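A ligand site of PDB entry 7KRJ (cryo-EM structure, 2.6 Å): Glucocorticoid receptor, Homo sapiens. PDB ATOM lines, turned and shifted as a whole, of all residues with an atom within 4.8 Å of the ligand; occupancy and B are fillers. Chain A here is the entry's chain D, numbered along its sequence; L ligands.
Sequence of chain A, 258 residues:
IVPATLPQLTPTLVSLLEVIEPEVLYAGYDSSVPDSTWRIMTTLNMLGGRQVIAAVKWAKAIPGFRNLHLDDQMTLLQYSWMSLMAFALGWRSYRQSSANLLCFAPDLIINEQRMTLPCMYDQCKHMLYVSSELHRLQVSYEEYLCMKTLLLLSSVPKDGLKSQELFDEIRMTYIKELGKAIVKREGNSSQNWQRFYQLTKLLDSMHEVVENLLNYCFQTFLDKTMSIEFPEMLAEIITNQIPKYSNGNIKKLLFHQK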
ATOM      1  N   MET A  41      23.739  16.334  10.161  1.00  0.00           N
ATOM      2  CA  MET A  41      24.545  16.057  11.315  1.00  0.00           C
ATOM      3  C   MET A  41      24.127  16.884  12.490  1.00  0.00           C
ATOM      4  O   MET A  41      24.114  16.354  13.600  1.00  0.00           O
ATOM      5  CB  MET A  41      25.999  16.239  10.992  1.00  0.00           C
ATOM      6  CG  MET A  41      26.495  15.132  10.113  1.00  0.00           C
ATOM      7  SD  MET A  41      28.250  15.135   9.839  1.00  0.00           S
ATOM      8  CE  MET A  41      28.378  16.395   8.580  1.00  0.00           C
ATOM      9  N   LEU A  44      21.175  15.268  14.084  1.00  0.00           N
ATOM     10  CA  LEU A  44      21.590  14.111  14.814  1.00  0.00           C
ATOM     11  C   LEU A  44      22.321  14.465  16.080  1.00  0.00           C
ATOM     12  O   LEU A  44      22.165  13.768  17.072  1.00  0.00           O
ATOM     13  CB  LEU A  44      22.468  13.234  13.941  1.00  0.00           C
ATOM     14  CG  LEU A  44      21.788  12.550  12.770  1.00  0.00           C
ATOM     15  CD1 LEU A  44      22.836  11.891  11.923  1.00  0.00           C
ATOM     16  CD2 LEU A  44      20.814  11.498  13.263  1.00  0.00           C
ATOM     17  N   ASN A  45      23.107  15.527  16.087  1.00  0.00           N
ATOM     18  CA  ASN A  45      23.826  15.848  17.291  1.00  0.00           C
ATOM     19  C   ASN A  45      22.868  16.289  18.368  1.00  0.00           C
ATOM     20  O   ASN A  45      23.043  15.968  19.544  1.00  0.00           O
ATOM     21  CB  ASN A  45      24.821  16.949  17.050  1.00  0.00           C
ATOM     22  CG  ASN A  45      25.953  16.494  16.237  1.00  0.00           C
ATOM     23  OD1 ASN A  45      26.279  15.315  16.160  1.00  0.00           O
ATOM     24  ND2 ASN A  45      26.571  17.418  15.597  1.00  0.00           N
ATOM     25  N   LEU A  47      19.826  15.322  18.692  1.00  0.00           N
ATOM     26  CA  LEU A  47      19.166  14.125  19.112  1.00  0.00           C
ATOM     27  C   LEU A  47      20.059  13.360  20.024  1.00  0.00           C
ATOM     28  O   LEU A  47      19.616  12.823  21.035  1.00  0.00           O
ATOM     29  CB  LEU A  47      18.805  13.260  17.932  1.00  0.00           C
ATOM     30  CG  LEU A  47      18.191  11.913  18.226  1.00  0.00           C
ATOM     31  CD1 LEU A  47      16.889  12.033  19.044  1.00  0.00           C
ATOM     32  CD2 LEU A  47      17.946  11.231  16.906  1.00  0.00           C
ATOM     33  N   GLY A  48      21.324  13.281  19.651  1.00  0.00           N
ATOM     34  CA  GLY A  48      22.301  12.545  20.405  1.00  0.00           C
ATOM     35  C   GLY A  48      22.376  13.111  21.784  1.00  0.00           C
ATOM     36  O   GLY A  48      22.527  12.361  22.754  1.00  0.00           O
ATOM     37  N   GLN A  51      19.532  11.778  23.711  1.00  0.00           N
ATOM     38  CA  GLN A  51      19.700  10.383  23.981  1.00  0.00           C
ATOM     39  C   GLN A  51      20.703  10.171  25.081  1.00  0.00           C
ATOM     40  O   GLN A  51      20.490   9.321  25.947  1.00  0.00           O
ATOM     41  CB  GLN A  51      20.141   9.657  22.751  1.00  0.00           C
ATOM     42  CG  GLN A  51      19.078   9.554  21.701  1.00  0.00           C
ATOM     43  CD  GLN A  51      19.644   8.977  20.494  1.00  0.00           C
ATOM     44  OE1 GLN A  51      20.870   8.940  20.424  1.00  0.00           O
ATOM     45  NE2 GLN A  51      18.832   8.530  19.543  1.00  0.00           N
ATOM     46  N   TRP A  81      30.081   6.405  26.218  1.00  0.00           N
ATOM     47  CA  TRP A  81      28.797   6.851  25.667  1.00  0.00           C
ATOM     48  C   TRP A  81      28.648   6.544  24.198  1.00  0.00           C
ATOM     49  O   TRP A  81      27.549   6.271  23.735  1.00  0.00           O
ATOM     50  CB  TRP A  81      28.546   8.327  25.871  1.00  0.00           C
ATOM     51  CG  TRP A  81      29.343   9.210  25.061  1.00  0.00           C
ATOM     52  CD1 TRP A  81      30.493   9.759  25.390  1.00  0.00           C
ATOM     53  CD2 TRP A  81      29.021   9.712  23.790  1.00  0.00           C
ATOM     54  NE1 TRP A  81      30.932  10.550  24.404  1.00  0.00           N
ATOM     55  CE2 TRP A  81      30.055  10.538  23.418  1.00  0.00           C
ATOM     56  CE3 TRP A  81      27.980   9.542  22.949  1.00  0.00           C
ATOM     57  CZ2 TRP A  81      30.059  11.197  22.252  1.00  0.00           C
ATOM     58  CZ3 TRP A  81      27.983  10.193  21.771  1.00  0.00           C
ATOM     59  CH2 TRP A  81      28.998  11.007  21.433  1.00  0.00           C
ATOM     60  N   MET A  82      29.737   6.523  23.467  1.00  0.00           N
ATOM     61  CA  MET A  82      29.605   6.257  22.063  1.00  0.00           C
ATOM     62  C   MET A  82      29.245   4.808  21.809  1.00  0.00           C
ATOM     63  O   MET A  82      28.613   4.494  20.804  1.00  0.00           O
ATOM     64  CB  MET A  82      30.870   6.609  21.344  1.00  0.00           C
ATOM     65  CG  MET A  82      30.789   6.502  19.837  1.00  0.00           C
ATOM     66  SD  MET A  82      29.608   7.595  19.124  1.00  0.00           S
ATOM     67  CE  MET A  82      30.581   9.062  18.956  1.00  0.00           C
ATOM     68  N   MET A  85      25.589   4.342  22.196  1.00  0.00           N
ATOM     69  CA  MET A  85      24.789   4.846  21.132  1.00  0.00           C
ATOM     70  C   MET A  85      24.879   3.979  19.897  1.00  0.00           C
ATOM     71  O   MET A  85      23.886   3.850  19.177  1.00  0.00           O
ATOM     72  CB  MET A  85      25.154   6.275  20.855  1.00  0.00           C
ATOM     73  CG  MET A  85      24.806   7.163  21.977  1.00  0.00           C
ATOM     74  SD  MET A  85      23.075   7.159  22.250  1.00  0.00           S
ATOM     75  CE  MET A  85      22.983   7.397  24.005  1.00  0.00           C
ATOM     76  N   ALA A  86      26.033   3.391  19.643  1.00  0.00           N
ATOM     77  CA  ALA A  86      26.136   2.527  18.488  1.00  0.00           C
ATOM     78  C   ALA A  86      25.202   1.333  18.625  1.00  0.00           C
ATOM     79  O   ALA A  86      24.529   0.965  17.673  1.00  0.00           O
ATOM     80  CB  ALA A  86      27.556   2.065  18.312  1.00  0.00           C
ATOM     81  N   LEU A  89      21.603   2.276  17.957  1.00  0.00           N
ATOM     82  CA  LEU A  89      21.341   2.414  16.542  1.00  0.00           C
ATOM     83  C   LEU A  89      21.235   1.074  15.893  1.00  0.00           C
ATOM     84  O   LEU A  89      20.329   0.843  15.089  1.00  0.00           O
ATOM     85  CB  LEU A  89      22.433   3.240  15.889  1.00  0.00           C
ATOM     86  CG  LEU A  89      22.301   3.536  14.392  1.00  0.00           C
ATOM     87  CD1 LEU A  89      21.028   4.269  14.104  1.00  0.00           C
ATOM     88  CD2 LEU A  89      23.473   4.375  13.968  1.00  0.00           C
ATOM     89  N   ARG A  92      17.960  -0.748  16.217  1.00  0.00           N
ATOM     90  CA  ARG A  92      16.750  -0.173  15.732  1.00  0.00           C
ATOM     91  C   ARG A  92      16.715  -0.502  14.285  1.00  0.00           C
ATOM     92  O   ARG A  92      15.653  -0.657  13.686  1.00  0.00           O
ATOM     93  CB  ARG A  92      16.675   1.318  15.922  1.00  0.00           C
ATOM     94  CG  ARG A  92      16.398   1.801  17.302  1.00  0.00           C
ATOM     95  CD  ARG A  92      16.097   3.264  17.300  1.00  0.00           C
ATOM     96  NE  ARG A  92      17.294   4.044  17.053  1.00  0.00           N
ATOM     97  CZ  ARG A  92      18.118   4.480  18.019  1.00  0.00           C
ATOM     98  NH1 ARG A  92      17.829   4.231  19.274  1.00  0.00           N
ATOM     99  NH2 ARG A  92      19.208   5.160  17.751  1.00  0.00           N
ATOM    100  N   PHE A 104      17.766   6.050  12.987  1.00  0.00           N
ATOM    101  CA  PHE A 104      18.284   6.875  14.064  1.00  0.00           C
ATOM    102  C   PHE A 104      17.163   7.194  14.986  1.00  0.00           C
ATOM    103  O   PHE A 104      17.311   7.253  16.202  1.00  0.00           O
ATOM    104  CB  PHE A 104      18.873   8.149  13.525  1.00  0.00           C
ATOM    105  CG  PHE A 104      20.110   7.933  12.822  1.00  0.00           C
ATOM    106  CD1 PHE A 104      20.102   7.734  11.476  1.00  0.00           C
ATOM    107  CD2 PHE A 104      21.283   7.933  13.494  1.00  0.00           C
ATOM    108  CE1 PHE A 104      21.272   7.537  10.824  1.00  0.00           C
ATOM    109  CE2 PHE A 104      22.450   7.749  12.842  1.00  0.00           C
ATOM    110  CZ  PHE A 104      22.451   7.553  11.510  1.00  0.00           C
ATOM    111  N   GLN A 123      31.922   6.208   7.234  1.00  0.00           N
ATOM    112  CA  GLN A 123      31.756   5.748   8.604  1.00  0.00           C
ATOM    113  C   GLN A 123      30.498   4.931   8.810  1.00  0.00           C
ATOM    114  O   GLN A 123      30.470   4.026   9.648  1.00  0.00           O
ATOM    115  CB  GLN A 123      31.790   6.939   9.544  1.00  0.00           C
ATOM    116  CG  GLN A 123      33.152   7.607   9.548  1.00  0.00           C
ATOM    117  CD  GLN A 123      34.212   6.659  10.053  1.00  0.00           C
ATOM    118  OE1 GLN A 123      34.116   6.167  11.188  1.00  0.00           O
ATOM    119  NE2 GLN A 123      35.198   6.349   9.217  1.00  0.00           N
ATOM    120  N   MET A 127      28.578   1.615  11.199  1.00  0.00           N
ATOM    121  CA  MET A 127      27.298   1.631  11.863  1.00  0.00           C
ATOM    122  C   MET A 127      26.438   0.492  11.341  1.00  0.00           C
ATOM    123  O   MET A 127      25.704  -0.170  12.091  1.00  0.00           O
ATOM    124  CB  MET A 127      26.628   2.978  11.666  1.00  0.00           C
ATOM    125  CG  MET A 127      27.361   4.084  12.393  1.00  0.00           C
ATOM    126  SD  MET A 127      26.491   5.657  12.453  1.00  0.00           S
ATOM    127  CE  MET A 127      26.655   6.277  10.849  1.00  0.00           C
ATOM    128  N   LEU A 213      34.503   5.972  14.946  1.00  0.00           N
ATOM    129  CA  LEU A 213      33.498   6.999  14.981  1.00  0.00           C
ATOM    130  C   LEU A 213      33.950   8.194  15.755  1.00  0.00           C
ATOM    131  O   LEU A 213      33.664   9.326  15.367  1.00  0.00           O
ATOM    132  CB  LEU A 213      32.242   6.452  15.629  1.00  0.00           C
ATOM    133  CG  LEU A 213      31.516   5.355  14.862  1.00  0.00           C
ATOM    134  CD1 LEU A 213      30.415   4.833  15.759  1.00  0.00           C
ATOM    135  CD2 LEU A 213      30.958   5.863  13.528  1.00  0.00           C
ATOM    136  N   TYR A 216      36.209  10.509  13.888  1.00  0.00           N
ATOM    137  CA  TYR A 216      35.465  11.378  13.026  1.00  0.00           C
ATOM    138  C   TYR A 216      34.791  12.482  13.843  1.00  0.00           C
ATOM    139  O   TYR A 216      34.805  13.646  13.472  1.00  0.00           O
ATOM    140  CB  TYR A 216      34.457  10.617  12.202  1.00  0.00           C
ATOM    141  CG  TYR A 216      33.793  11.550  11.303  1.00  0.00           C
ATOM    142  CD1 TYR A 216      34.450  11.960  10.181  1.00  0.00           C
ATOM    143  CD2 TYR A 216      32.562  12.039  11.592  1.00  0.00           C
ATOM    144  CE1 TYR A 216      33.883  12.873   9.363  1.00  0.00           C
ATOM    145  CE2 TYR A 216      31.978  12.948  10.777  1.00  0.00           C
ATOM    146  CZ  TYR A 216      32.637  13.380   9.658  1.00  0.00           C
ATOM    147  OH  TYR A 216      32.062  14.314   8.828  1.00  0.00           O
ATOM    148  N   CYS A 217      34.171  12.104  14.951  1.00  0.00           N
ATOM    149  CA  CYS A 217      33.475  13.057  15.798  1.00  0.00           C
ATOM    150  C   CYS A 217      34.340  14.183  16.244  1.00  0.00           C
ATOM    151  O   CYS A 217      33.935  15.342  16.223  1.00  0.00           O
ATOM    152  CB  CYS A 217      32.956  12.406  17.070  1.00  0.00           C
ATOM    153  SG  CYS A 217      32.136  13.576  18.149  1.00  0.00           S
ATOM    154  N   THR A 220      34.879  16.709  13.452  1.00  0.00           N
ATOM    155  CA  THR A 220      33.827  17.681  13.116  1.00  0.00           C
ATOM    156  C   THR A 220      33.556  18.603  14.262  1.00  0.00           C
ATOM    157  O   THR A 220      33.180  19.756  14.066  1.00  0.00           O
ATOM    158  CB  THR A 220      32.488  17.025  12.775  1.00  0.00           C
ATOM    159  OG1 THR A 220      32.056  16.250  13.885  1.00  0.00           O
ATOM    160  CG2 THR A 220      32.618  16.169  11.589  1.00  0.00           C
ATOM    161  N   ILE A 228      28.397  22.506  11.870  1.00  0.00           N
ATOM    162  CA  ILE A 228      27.905  21.380  12.627  1.00  0.00           C
ATOM    163  C   ILE A 228      27.807  21.770  14.069  1.00  0.00           C
ATOM    164  O   ILE A 228      28.818  21.991  14.730  1.00  0.00           O
ATOM    165  CB  ILE A 228      28.844  20.190  12.439  1.00  0.00           C
ATOM    166  CG1 ILE A 228      28.917  19.859  10.927  1.00  0.00           C
ATOM    167  CG2 ILE A 228      28.333  19.008  13.258  1.00  0.00           C
ATOM    168  CD1 ILE A 228      30.004  18.889  10.541  1.00  0.00           C
ATOM    169  N   PHE A 230      26.552  21.389  18.150  1.00  0.00           N
ATOM    170  CA  PHE A 230      26.411  20.418  19.195  1.00  0.00           C
ATOM    171  C   PHE A 230      25.633  21.000  20.339  1.00  0.00           C
ATOM    172  O   PHE A 230      25.669  22.206  20.533  1.00  0.00           O
ATOM    173  CB  PHE A 230      27.787  20.003  19.678  1.00  0.00           C
ATOM    174  CG  PHE A 230      28.553  19.316  18.659  1.00  0.00           C
ATOM    175  CD1 PHE A 230      29.212  20.011  17.676  1.00  0.00           C
ATOM    176  CD2 PHE A 230      28.629  17.949  18.667  1.00  0.00           C
ATOM    177  CE1 PHE A 230      29.905  19.378  16.721  1.00  0.00           C
ATOM    178  CE2 PHE A 230      29.350  17.302  17.710  1.00  0.00           C
ATOM    179  CZ  PHE A 230      29.986  18.019  16.731  1.00  0.00           C
HETATM  180  C1  LIG L   1      22.744  10.310  17.478  1.00  0.00           C
HETATM  181  C2  LIG L   1      21.569   9.660  17.432  1.00  0.00           C
HETATM  182  C3  LIG L   1      21.603   8.121  17.383  1.00  0.00           C
HETATM  183  C4  LIG L   1      22.942   7.398  17.385  1.00  0.00           C
HETATM  184  C5  LIG L   1      24.087   8.113  17.426  1.00  0.00           C
HETATM  185  C6  LIG L   1      25.389   7.336  17.396  1.00  0.00           C
HETATM  186  C7  LIG L   1      26.349   7.874  16.324  1.00  0.00           C
HETATM  187  C8  LIG L   1      26.408   9.407  16.161  1.00  0.00           C
HETATM  188  C9  LIG L   1      25.050  10.199  16.310  1.00  0.00           C
HETATM  189  C10 LIG L   1      24.148   9.669  17.482  1.00  0.00           C
HETATM  190  C11 LIG L   1      25.181  11.728  16.110  1.00  0.00           C
HETATM  191  C12 LIG L   1      26.250  12.250  15.124  1.00  0.00           C
HETATM  192  C13 LIG L   1      27.592  11.483  15.144  1.00  0.00           C
HETATM  193  C14 LIG L   1      27.341   9.938  15.044  1.00  0.00           C
HETATM  194  C15 LIG L   1      28.704   9.330  14.721  1.00  0.00           C
HETATM  195  C16 LIG L   1      29.389  10.395  13.863  1.00  0.00           C
HETATM  196  C17 LIG L   1      28.469  11.635  13.868  1.00  0.00           C
HETATM  197  C18 LIG L   1      28.340  11.914  16.436  1.00  0.00           C
HETATM  198  C19 LIG L   1      24.668  10.012  18.878  1.00  0.00           C
HETATM  199  C20 LIG L   1      29.229  12.982  13.731  1.00  0.00           C
HETATM  200  C21 LIG L   1      28.524  14.284  13.331  1.00  0.00           C
HETATM  201  C22 LIG L   1      29.826   9.800  12.525  1.00  0.00           C
HETATM  202  F1  LIG L   1      24.370   9.887  15.156  1.00  0.00           F
HETATM  203  O1  LIG L   1      20.556   7.489  17.359  1.00  0.00           O
HETATM  204  O2  LIG L   1      25.436  12.362  17.342  1.00  0.00           O
HETATM  205  O3  LIG L   1      27.626  11.515  12.722  1.00  0.00           O
HETATM  206  O4  LIG L   1      30.432  13.033  13.975  1.00  0.00           O
HETATM  207  O5  LIG L   1      29.264  15.472  13.647  1.00  0.00           O
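NE2 of Gln 51 is in hydrogen-bond range of O1 of the ligand, 3.0 Å away. An oxygen (O1) of the ligand sits at hydrogen-bond distance from the guanidinium group (NH2) of Arg 92 (2.7 Å). O2 of the ligand sits close to OD1 of Asn 45, at 3.3 Å. An oxygen (O5) of the ligand is in hydrogen-bond range of the side-chain hydroxyl of Thr 220, at 2.9 Å.
The backbone carbonyl oxygen of Phe 104 sits at hydrogen-bond distance from the guanidinium group of Arg 92 (3.2 Å). The side-chain amide oxygen (OE1) of Gln 51 sits close to the side-chain sulfur (SD) of Met 85. The side-chain hydroxyl of Thr 220 sits at hydrogen-bond distance from the backbone carbonyl oxygen of Cys 217 (3.1 Å). The side-chain amide nitrogen of Asn 45 lies close to the backbone carbonyl oxygen of Met 41 (3.3 Å).
The backbone carbonyl oxygen of Phe 104 lies close to an oxygen (O1) of the ligand (3.5 Å). Merely in contact with the ligand: Met 41, Leu 44, Leu 47, Gly 48, Met 85, Tyr 216, Cys 217 and Ile 228. 13 residues have an atom within 4 Å of the ligand: Met 41, Leu 44, Asn 45, Leu 47, Gly 48, Gln 51, Met 85, Arg 92, Phe 104, Tyr 216, Cys 217, Thr 220 and Ile 228. The nearest printed residue that does not touch the ligand is Phe 230 (4.1 Å).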
